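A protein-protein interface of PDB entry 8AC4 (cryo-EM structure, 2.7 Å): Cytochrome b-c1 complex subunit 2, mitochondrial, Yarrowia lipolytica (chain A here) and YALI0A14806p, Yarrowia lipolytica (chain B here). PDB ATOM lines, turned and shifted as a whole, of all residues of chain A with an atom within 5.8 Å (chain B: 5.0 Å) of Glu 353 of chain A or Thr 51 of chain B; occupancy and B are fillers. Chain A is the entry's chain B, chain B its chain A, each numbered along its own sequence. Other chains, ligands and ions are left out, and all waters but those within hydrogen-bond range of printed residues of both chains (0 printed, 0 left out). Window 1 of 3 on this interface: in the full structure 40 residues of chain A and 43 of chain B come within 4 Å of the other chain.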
ATOM      1  N   ASN A 196      12.967  -0.522 -15.862  1.00  0.00           N
ATOM      2  CA  ASN A 196      13.507  -0.205 -17.175  1.00  0.00           C
ATOM      3  C   ASN A 196      13.801  -1.477 -17.972  1.00  0.00           C
ATOM      4  O   ASN A 196      14.637  -2.288 -17.571  1.00  0.00           O
ATOM      5  CB  ASN A 196      14.796   0.596 -17.034  1.00  0.00           C
ATOM      6  CG  ASN A 196      14.912   1.629 -18.128  1.00  0.00           C
ATOM      7  OD1 ASN A 196      14.815   1.311 -19.312  1.00  0.00           O
ATOM      8  ND2 ASN A 196      15.067   2.884 -17.738  1.00  0.00           N
ATOM      9  N   PHE A 346      19.101  19.026 -23.293  1.00  0.00           N
ATOM     10  CA  PHE A 346      20.074  17.959 -23.330  1.00  0.00           C
ATOM     11  C   PHE A 346      20.271  17.411 -21.927  1.00  0.00           C
ATOM     12  O   PHE A 346      20.336  16.200 -21.757  1.00  0.00           O
ATOM     13  CB  PHE A 346      21.422  18.427 -23.875  1.00  0.00           C
ATOM     14  CG  PHE A 346      22.441  17.317 -23.911  1.00  0.00           C
ATOM     15  CD1 PHE A 346      22.358  16.321 -24.878  1.00  0.00           C
ATOM     16  CD2 PHE A 346      23.465  17.247 -22.974  1.00  0.00           C
ATOM     17  CE1 PHE A 346      23.287  15.291 -24.920  1.00  0.00           C
ATOM     18  CE2 PHE A 346      24.400  16.221 -23.027  1.00  0.00           C
ATOM     19  CZ  PHE A 346      24.306  15.242 -23.993  1.00  0.00           C
ATOM     20  N   ALA A 348      18.243  17.355 -19.539  1.00  0.00           N
ATOM     21  CA  ALA A 348      17.056  16.618 -19.137  1.00  0.00           C
ATOM     22  C   ALA A 348      17.074  15.222 -19.750  1.00  0.00           C
ATOM     23  O   ALA A 348      16.735  14.258 -19.069  1.00  0.00           O
ATOM     24  CB  ALA A 348      15.802  17.361 -19.519  1.00  0.00           C
ATOM     25  N   ALA A 349      17.498  15.135 -21.016  1.00  0.00           N
ATOM     26  CA  ALA A 349      17.465  13.883 -21.756  1.00  0.00           C
ATOM     27  C   ALA A 349      18.448  12.887 -21.148  1.00  0.00           C
ATOM     28  O   ALA A 349      18.067  11.760 -20.849  1.00  0.00           O
ATOM     29  CB  ALA A 349      17.744  14.129 -23.214  1.00  0.00           C
ATOM     30  N   GLU A 350      19.688  13.330 -20.917  1.00  0.00           N
ATOM     31  CA  GLU A 350      20.742  12.466 -20.407  1.00  0.00           C
ATOM     32  C   GLU A 350      20.455  12.022 -18.969  1.00  0.00           C
ATOM     33  O   GLU A 350      20.911  10.959 -18.550  1.00  0.00           O
ATOM     34  CB  GLU A 350      22.105  13.126 -20.613  1.00  0.00           C
ATOM     35  CG  GLU A 350      22.377  14.281 -19.664  1.00  0.00           C
ATOM     36  CD  GLU A 350      23.702  15.008 -19.841  1.00  0.00           C
ATOM     37  OE1 GLU A 350      23.746  16.221 -19.560  1.00  0.00           O
ATOM     38  OE2 GLU A 350      24.705  14.366 -20.235  1.00  0.00           O
ATOM     39  N   ALA A 351      19.687  12.828 -18.221  1.00  0.00           N
ATOM     40  CA  ALA A 351      19.309  12.476 -16.858  1.00  0.00           C
ATOM     41  C   ALA A 351      18.300  11.332 -16.882  1.00  0.00           C
ATOM     42  O   ALA A 351      18.356  10.422 -16.062  1.00  0.00           O
ATOM     43  CB  ALA A 351      18.761  13.682 -16.134  1.00  0.00           C
ATOM     44  N   PHE A 352      17.383  11.379 -17.844  1.00  0.00           N
ATOM     45  CA  PHE A 352      16.360  10.362 -17.972  1.00  0.00           C
ATOM     46  C   PHE A 352      16.931   9.091 -18.600  1.00  0.00           C
ATOM     47  O   PHE A 352      16.265   8.061 -18.630  1.00  0.00           O
ATOM     48  CB  PHE A 352      15.195  10.970 -18.747  1.00  0.00           C
ATOM     49  CG  PHE A 352      13.912  10.193 -18.672  1.00  0.00           C
ATOM     50  CD1 PHE A 352      13.371   9.802 -17.451  1.00  0.00           C
ATOM     51  CD2 PHE A 352      13.239   9.861 -19.838  1.00  0.00           C
ATOM     52  CE1 PHE A 352      12.188   9.082 -17.409  1.00  0.00           C
ATOM     53  CE2 PHE A 352      12.044   9.157 -19.791  1.00  0.00           C
ATOM     54  CZ  PHE A 352      11.515   8.782 -18.574  1.00  0.00           C
ATOM     55  N   GLU A 353      18.184   9.152 -19.073  1.00  0.00           N
ATOM     56  CA  GLU A 353      18.855   7.990 -19.641  1.00  0.00           C
ATOM     57  C   GLU A 353      19.661   7.261 -18.569  1.00  0.00           C
ATOM     58  O   GLU A 353      19.519   6.051 -18.430  1.00  0.00           O
ATOM     59  CB  GLU A 353      19.705   8.358 -20.858  1.00  0.00           C
ATOM     60  CG  GLU A 353      18.881   8.518 -22.122  1.00  0.00           C
ATOM     61  CD  GLU A 353      19.242   9.696 -23.007  1.00  0.00           C
ATOM     62  OE1 GLU A 353      20.396  10.166 -22.931  1.00  0.00           O
ATOM     63  OE2 GLU A 353      18.390  10.083 -23.833  1.00  0.00           O
ATOM     64  N   ASN A 354      20.508   7.997 -17.836  1.00  0.00           N
ATOM     65  CA  ASN A 354      21.298   7.452 -16.739  1.00  0.00           C
ATOM     66  C   ASN A 354      20.388   6.724 -15.746  1.00  0.00           C
ATOM     67  O   ASN A 354      19.497   7.349 -15.173  1.00  0.00           O
ATOM     68  CB  ASN A 354      22.122   8.530 -16.022  1.00  0.00           C
ATOM     69  CG  ASN A 354      22.845   8.009 -14.798  1.00  0.00           C
ATOM     70  OD1 ASN A 354      23.657   7.096 -14.929  1.00  0.00           O
ATOM     71  ND2 ASN A 354      22.583   8.590 -13.630  1.00  0.00           N
ATOM     72  N   PRO A 355      20.581   5.402 -15.499  1.00  0.00           N
ATOM     73  CA  PRO A 355      19.646   4.623 -14.681  1.00  0.00           C
ATOM     74  C   PRO A 355      19.461   5.145 -13.259  1.00  0.00           C
ATOM     75  O   PRO A 355      18.351   5.076 -12.735  1.00  0.00           O
ATOM     76  CB  PRO A 355      20.263   3.220 -14.651  1.00  0.00           C
ATOM     77  CG  PRO A 355      21.123   3.164 -15.890  1.00  0.00           C
ATOM     78  CD  PRO A 355      21.677   4.567 -16.019  1.00  0.00           C
ATOM     79  N   SER A 357      19.585   8.296 -12.083  1.00  0.00           N
ATOM     80  CA  SER A 357      18.737   9.474 -12.027  1.00  0.00           C
ATOM     81  C   SER A 357      17.358   9.171 -12.603  1.00  0.00           C
ATOM     82  O   SER A 357      16.360   9.693 -12.108  1.00  0.00           O
ATOM     83  CB  SER A 357      19.379  10.670 -12.677  1.00  0.00           C
ATOM     84  OG  SER A 357      20.082  10.306 -13.853  1.00  0.00           O
ATOM     85  N   SER A 358      17.314   8.289 -13.611  1.00  0.00           N
ATOM     86  CA  SER A 358      16.058   7.906 -14.235  1.00  0.00           C
ATOM     87  C   SER A 358      15.073   7.417 -13.174  1.00  0.00           C
ATOM     88  O   SER A 358      13.947   7.915 -13.076  1.00  0.00           O
ATOM     89  CB  SER A 358      16.267   6.866 -15.303  1.00  0.00           C
ATOM     90  OG  SER A 358      15.044   6.654 -16.015  1.00  0.00           O
ATOM     91  N   VAL B  49      15.422   6.062 -26.547  1.00  0.00           N
ATOM     92  CA  VAL B  49      16.213   7.172 -26.032  1.00  0.00           C
ATOM     93  C   VAL B  49      16.040   8.386 -26.940  1.00  0.00           C
ATOM     94  O   VAL B  49      15.515   8.278 -28.050  1.00  0.00           O
ATOM     95  CB  VAL B  49      17.704   6.823 -25.835  1.00  0.00           C
ATOM     96  CG1 VAL B  49      17.930   5.764 -24.766  1.00  0.00           C
ATOM     97  CG2 VAL B  49      18.398   6.458 -27.140  1.00  0.00           C
ATOM     98  N   GLN B  50      16.520   9.533 -26.450  1.00  0.00           N
ATOM     99  CA  GLN B  50      16.282  10.811 -27.096  1.00  0.00           C
ATOM    100  C   GLN B  50      17.609  11.471 -27.453  1.00  0.00           C
ATOM    101  O   GLN B  50      17.625  12.461 -28.185  1.00  0.00           O
ATOM    102  CB  GLN B  50      15.380  11.685 -26.222  1.00  0.00           C
ATOM    103  CG  GLN B  50      13.901  11.540 -26.559  1.00  0.00           C
ATOM    104  CD  GLN B  50      13.250  12.823 -27.015  1.00  0.00           C
ATOM    105  OE1 GLN B  50      12.987  13.718 -26.216  1.00  0.00           O
ATOM    106  NE2 GLN B  50      12.963  12.919 -28.305  1.00  0.00           N
ATOM    107  N   THR B  51      18.706  10.898 -26.947  1.00  0.00           N
ATOM    108  CA  THR B  51      20.043  11.366 -27.270  1.00  0.00           C
ATOM    109  C   THR B  51      20.682  10.448 -28.306  1.00  0.00           C
ATOM    110  O   THR B  51      20.195   9.345 -28.508  1.00  0.00           O
ATOM    111  CB  THR B  51      20.962  11.435 -26.044  1.00  0.00           C
ATOM    112  OG1 THR B  51      21.222  10.161 -25.446  1.00  0.00           O
ATOM    113  CG2 THR B  51      20.613  12.534 -25.062  1.00  0.00           C
ATOM    114  N   ALA B  52      21.753  10.922 -28.953  1.00  0.00           N
ATOM    115  CA  ALA B  52      22.551  10.099 -29.852  1.00  0.00           C
ATOM    116  C   ALA B  52      24.036  10.325 -29.583  1.00  0.00           C
ATOM    117  O   ALA B  52      24.463  11.457 -29.362  1.00  0.00           O
ATOM    118  CB  ALA B  52      22.233  10.440 -31.291  1.00  0.00           C
ATOM    119  N   THR B  53      24.846   9.266 -29.701  1.00  0.00           N
ATOM    120  CA  THR B  53      26.294   9.417 -29.731  1.00  0.00           C
ATOM    121  C   THR B  53      26.794   9.093 -31.135  1.00  0.00           C
ATOM    122  O   THR B  53      26.749   7.935 -31.527  1.00  0.00           O
ATOM    123  CB  THR B  53      26.960   8.511 -28.689  1.00  0.00           C
ATOM    124  OG1 THR B  53      26.444   8.877 -27.413  1.00  0.00           O
ATOM    125  CG2 THR B  53      28.467   8.636 -28.675  1.00  0.00           C
ATOM    126  N   LYS B 117      28.142  13.551 -28.160  1.00  0.00           N
ATOM    127  CA  LYS B 117      26.837  13.219 -27.620  1.00  0.00           C
ATOM    128  C   LYS B 117      25.935  14.430 -27.811  1.00  0.00           C
ATOM    129  O   LYS B 117      26.325  15.536 -27.465  1.00  0.00           O
ATOM    130  CB  LYS B 117      26.964  12.838 -26.147  1.00  0.00           C
ATOM    131  CG  LYS B 117      25.838  11.942 -25.667  1.00  0.00           C
ATOM    132  CD  LYS B 117      26.008  11.393 -24.281  1.00  0.00           C
ATOM    133  CE  LYS B 117      24.747  10.675 -23.840  1.00  0.00           C
ATOM    134  NZ  LYS B 117      24.940   9.208 -23.794  1.00  0.00           N
ATOM    135  N   SER B 118      24.752  14.212 -28.385  1.00  0.00           N
ATOM    136  CA  SER B 118      23.862  15.315 -28.695  1.00  0.00           C
ATOM    137  C   SER B 118      22.409  14.890 -28.526  1.00  0.00           C
ATOM    138  O   SER B 118      22.115  13.822 -28.004  1.00  0.00           O
ATOM    139  CB  SER B 118      24.116  15.841 -30.087  1.00  0.00           C
ATOM    140  OG  SER B 118      23.848  14.834 -31.049  1.00  0.00           O
ATOM    141  N   PHE B 119      21.517  15.780 -28.952  1.00  0.00           N
ATOM    142  CA  PHE B 119      20.108  15.481 -29.055  1.00  0.00           C
ATOM    143  C   PHE B 119      19.844  14.825 -30.407  1.00  0.00           C
ATOM    144  O   PHE B 119      20.723  14.822 -31.262  1.00  0.00           O
ATOM    145  CB  PHE B 119      19.316  16.756 -28.785  1.00  0.00           C
ATOM    146  CG  PHE B 119      18.029  16.443 -28.084  1.00  0.00           C
ATOM    147  CD1 PHE B 119      18.034  16.116 -26.738  1.00  0.00           C
ATOM    148  CD2 PHE B 119      16.840  16.354 -28.796  1.00  0.00           C
ATOM    149  CE1 PHE B 119      16.853  15.764 -26.104  1.00  0.00           C
ATOM    150  CE2 PHE B 119      15.661  16.001 -28.160  1.00  0.00           C
ATOM    151  CZ  PHE B 119      15.671  15.705 -26.814  1.00  0.00           C
ATOM    152  N   LYS B 120      18.653  14.242 -30.571  1.00  0.00           N
ATOM    153  CA  LYS B 120      18.312  13.433 -31.732  1.00  0.00           C
ATOM    154  C   LYS B 120      18.518  14.212 -33.035  1.00  0.00           C
ATOM    155  O   LYS B 120      19.058  13.681 -34.008  1.00  0.00           O
ATOM    156  CB  LYS B 120      16.875  12.913 -31.595  1.00  0.00           C
ATOM    157  CG  LYS B 120      16.334  12.187 -32.824  1.00  0.00           C
ATOM    158  CD  LYS B 120      14.817  12.227 -32.985  1.00  0.00           C
ATOM    159  CE  LYS B 120      14.317  11.517 -34.230  1.00  0.00           C
ATOM    160  NZ  LYS B 120      12.839  11.568 -34.358  1.00  0.00           N
ATOM    161  N   ALA B 217      25.048   5.608 -32.258  1.00  0.00           N
ATOM    162  CA  ALA B 217      24.200   4.842 -31.364  1.00  0.00           C
ATOM    163  C   ALA B 217      23.150   5.753 -30.739  1.00  0.00           C
ATOM    164  O   ALA B 217      23.440   6.895 -30.384  1.00  0.00           O
ATOM    165  CB  ALA B 217      25.041   4.181 -30.305  1.00  0.00           C
ATOM    166  N   GLY B 218      21.953   5.198 -30.529  1.00  0.00           N
ATOM    167  CA  GLY B 218      20.866   5.920 -29.894  1.00  0.00           C
ATOM    168  C   GLY B 218      19.844   6.339 -30.937  1.00  0.00           C
ATOM    169  O   GLY B 218      19.463   5.553 -31.794  1.00  0.00           O
ATOM    170  N   ALA B 219      19.441   7.602 -30.877  1.00  0.00           N
ATOM    171  CA  ALA B 219      18.412   8.083 -31.775  1.00  0.00           C
ATOM    172  C   ALA B 219      19.042   8.542 -33.090  1.00  0.00           C
ATOM    173  O   ALA B 219      19.143   9.738 -33.356  1.00  0.00           O
ATOM    174  CB  ALA B 219      17.640   9.169 -31.075  1.00  0.00           C
ATOM    175  N   THR B 400      24.136   5.196 -24.474  1.00  0.00           N
ATOM    176  CA  THR B 400      24.461   5.272 -25.895  1.00  0.00           C
ATOM    177  C   THR B 400      25.966   5.372 -26.113  1.00  0.00           C
ATOM    178  O   THR B 400      26.466   4.895 -27.129  1.00  0.00           O
ATOM    179  CB  THR B 400      23.763   6.410 -26.645  1.00  0.00           C
ATOM    180  OG1 THR B 400      24.297   7.645 -26.163  1.00  0.00           O
ATOM    181  CG2 THR B 400      22.262   6.351 -26.502  1.00  0.00           C
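Printed residues of chain B within 4 Å of Phe 346 of chain A: Thr 51 (3.8 Å), Lys 117 (3.97 Å) and Ser 118 (3.6 Å).
Glu 350 of chain A touches none of the printed residues of chain B.
Thr 51 of chain B touches three residues of chain A.
Of the printed residues of chain A, Lys 117 of chain B touches Phe 346.
Of the printed residues of chain A, Ser 118 of chain B touches Phe 346.
Printed residues of chain A within 4 Å of Phe 119 of chain B: Ala 349 (3.4 Å).
Lys 120 of chain B touches none of the printed residues of chain A.
The nearest residue of chain B that does not touch Glu 353 of chain A is Lys 117 of chain B (4.5 Å).
The nearest residue of chain A that does not touch Thr 51 of chain B is Glu 350 of chain A (4.3 Å).
The nearest printed residue of chain A that does not touch Phe 119 of chain B is Phe 346 of chain A (4.2 Å).
Printed residues of chain B that touch a printed residue of chain A: Val 49, Gln 50, Thr 51, Lys 117, Ser 118 and Phe 119.
The backbone NH (N) of Gln 50 of chain B lies within hydrogen-bond range of the side-chain carboxylate (OE2) of Glu 353 of chain A.
The side-chain hydroxyl of Thr 51 of chain B sits at hydrogen-bond distance from the side-chain carboxylate of Glu 353 of chain A (2.6 Å).
Thr 51 of chain B touches Phe 346 of chain A (CG2 to CE1, 3.8 Å).
Lys 117 of chain B touches Phe 346 of chain A (O to CE1, 3.97 Å).
Phe 346 of chain A touches Ser 118 of chain B.
Ala 349 of chain A touches Thr 51 of chain B (CB to CG2, 3.8 Å).
Ala 349 of chain A touches Phe 119 of chain B (CB to CE1, 3.4 Å).
Glu 353 of chain A touches Val 49 of chain B (OE2 to CB, 3.9 Å).
N of Lys 120 of chain B sits at hydrogen-bond distance from O of Gln 50 of chain B, 3.1 Å away.
The backbone carbonyl oxygen (O) of Thr 51 of chain B is in hydrogen-bond range of the backbone NH (N) of Ala 219 of chain B.
N of Ser 118 of chain B lies within hydrogen-bond range of O of Ala 52 of chain B (2.9 Å).
The side-chain amino group (NZ) of Lys 117 of chain B sits at hydrogen-bond distance from the side-chain hydroxyl (OG1) of Thr 400 of chain B, 2.9 Å away.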
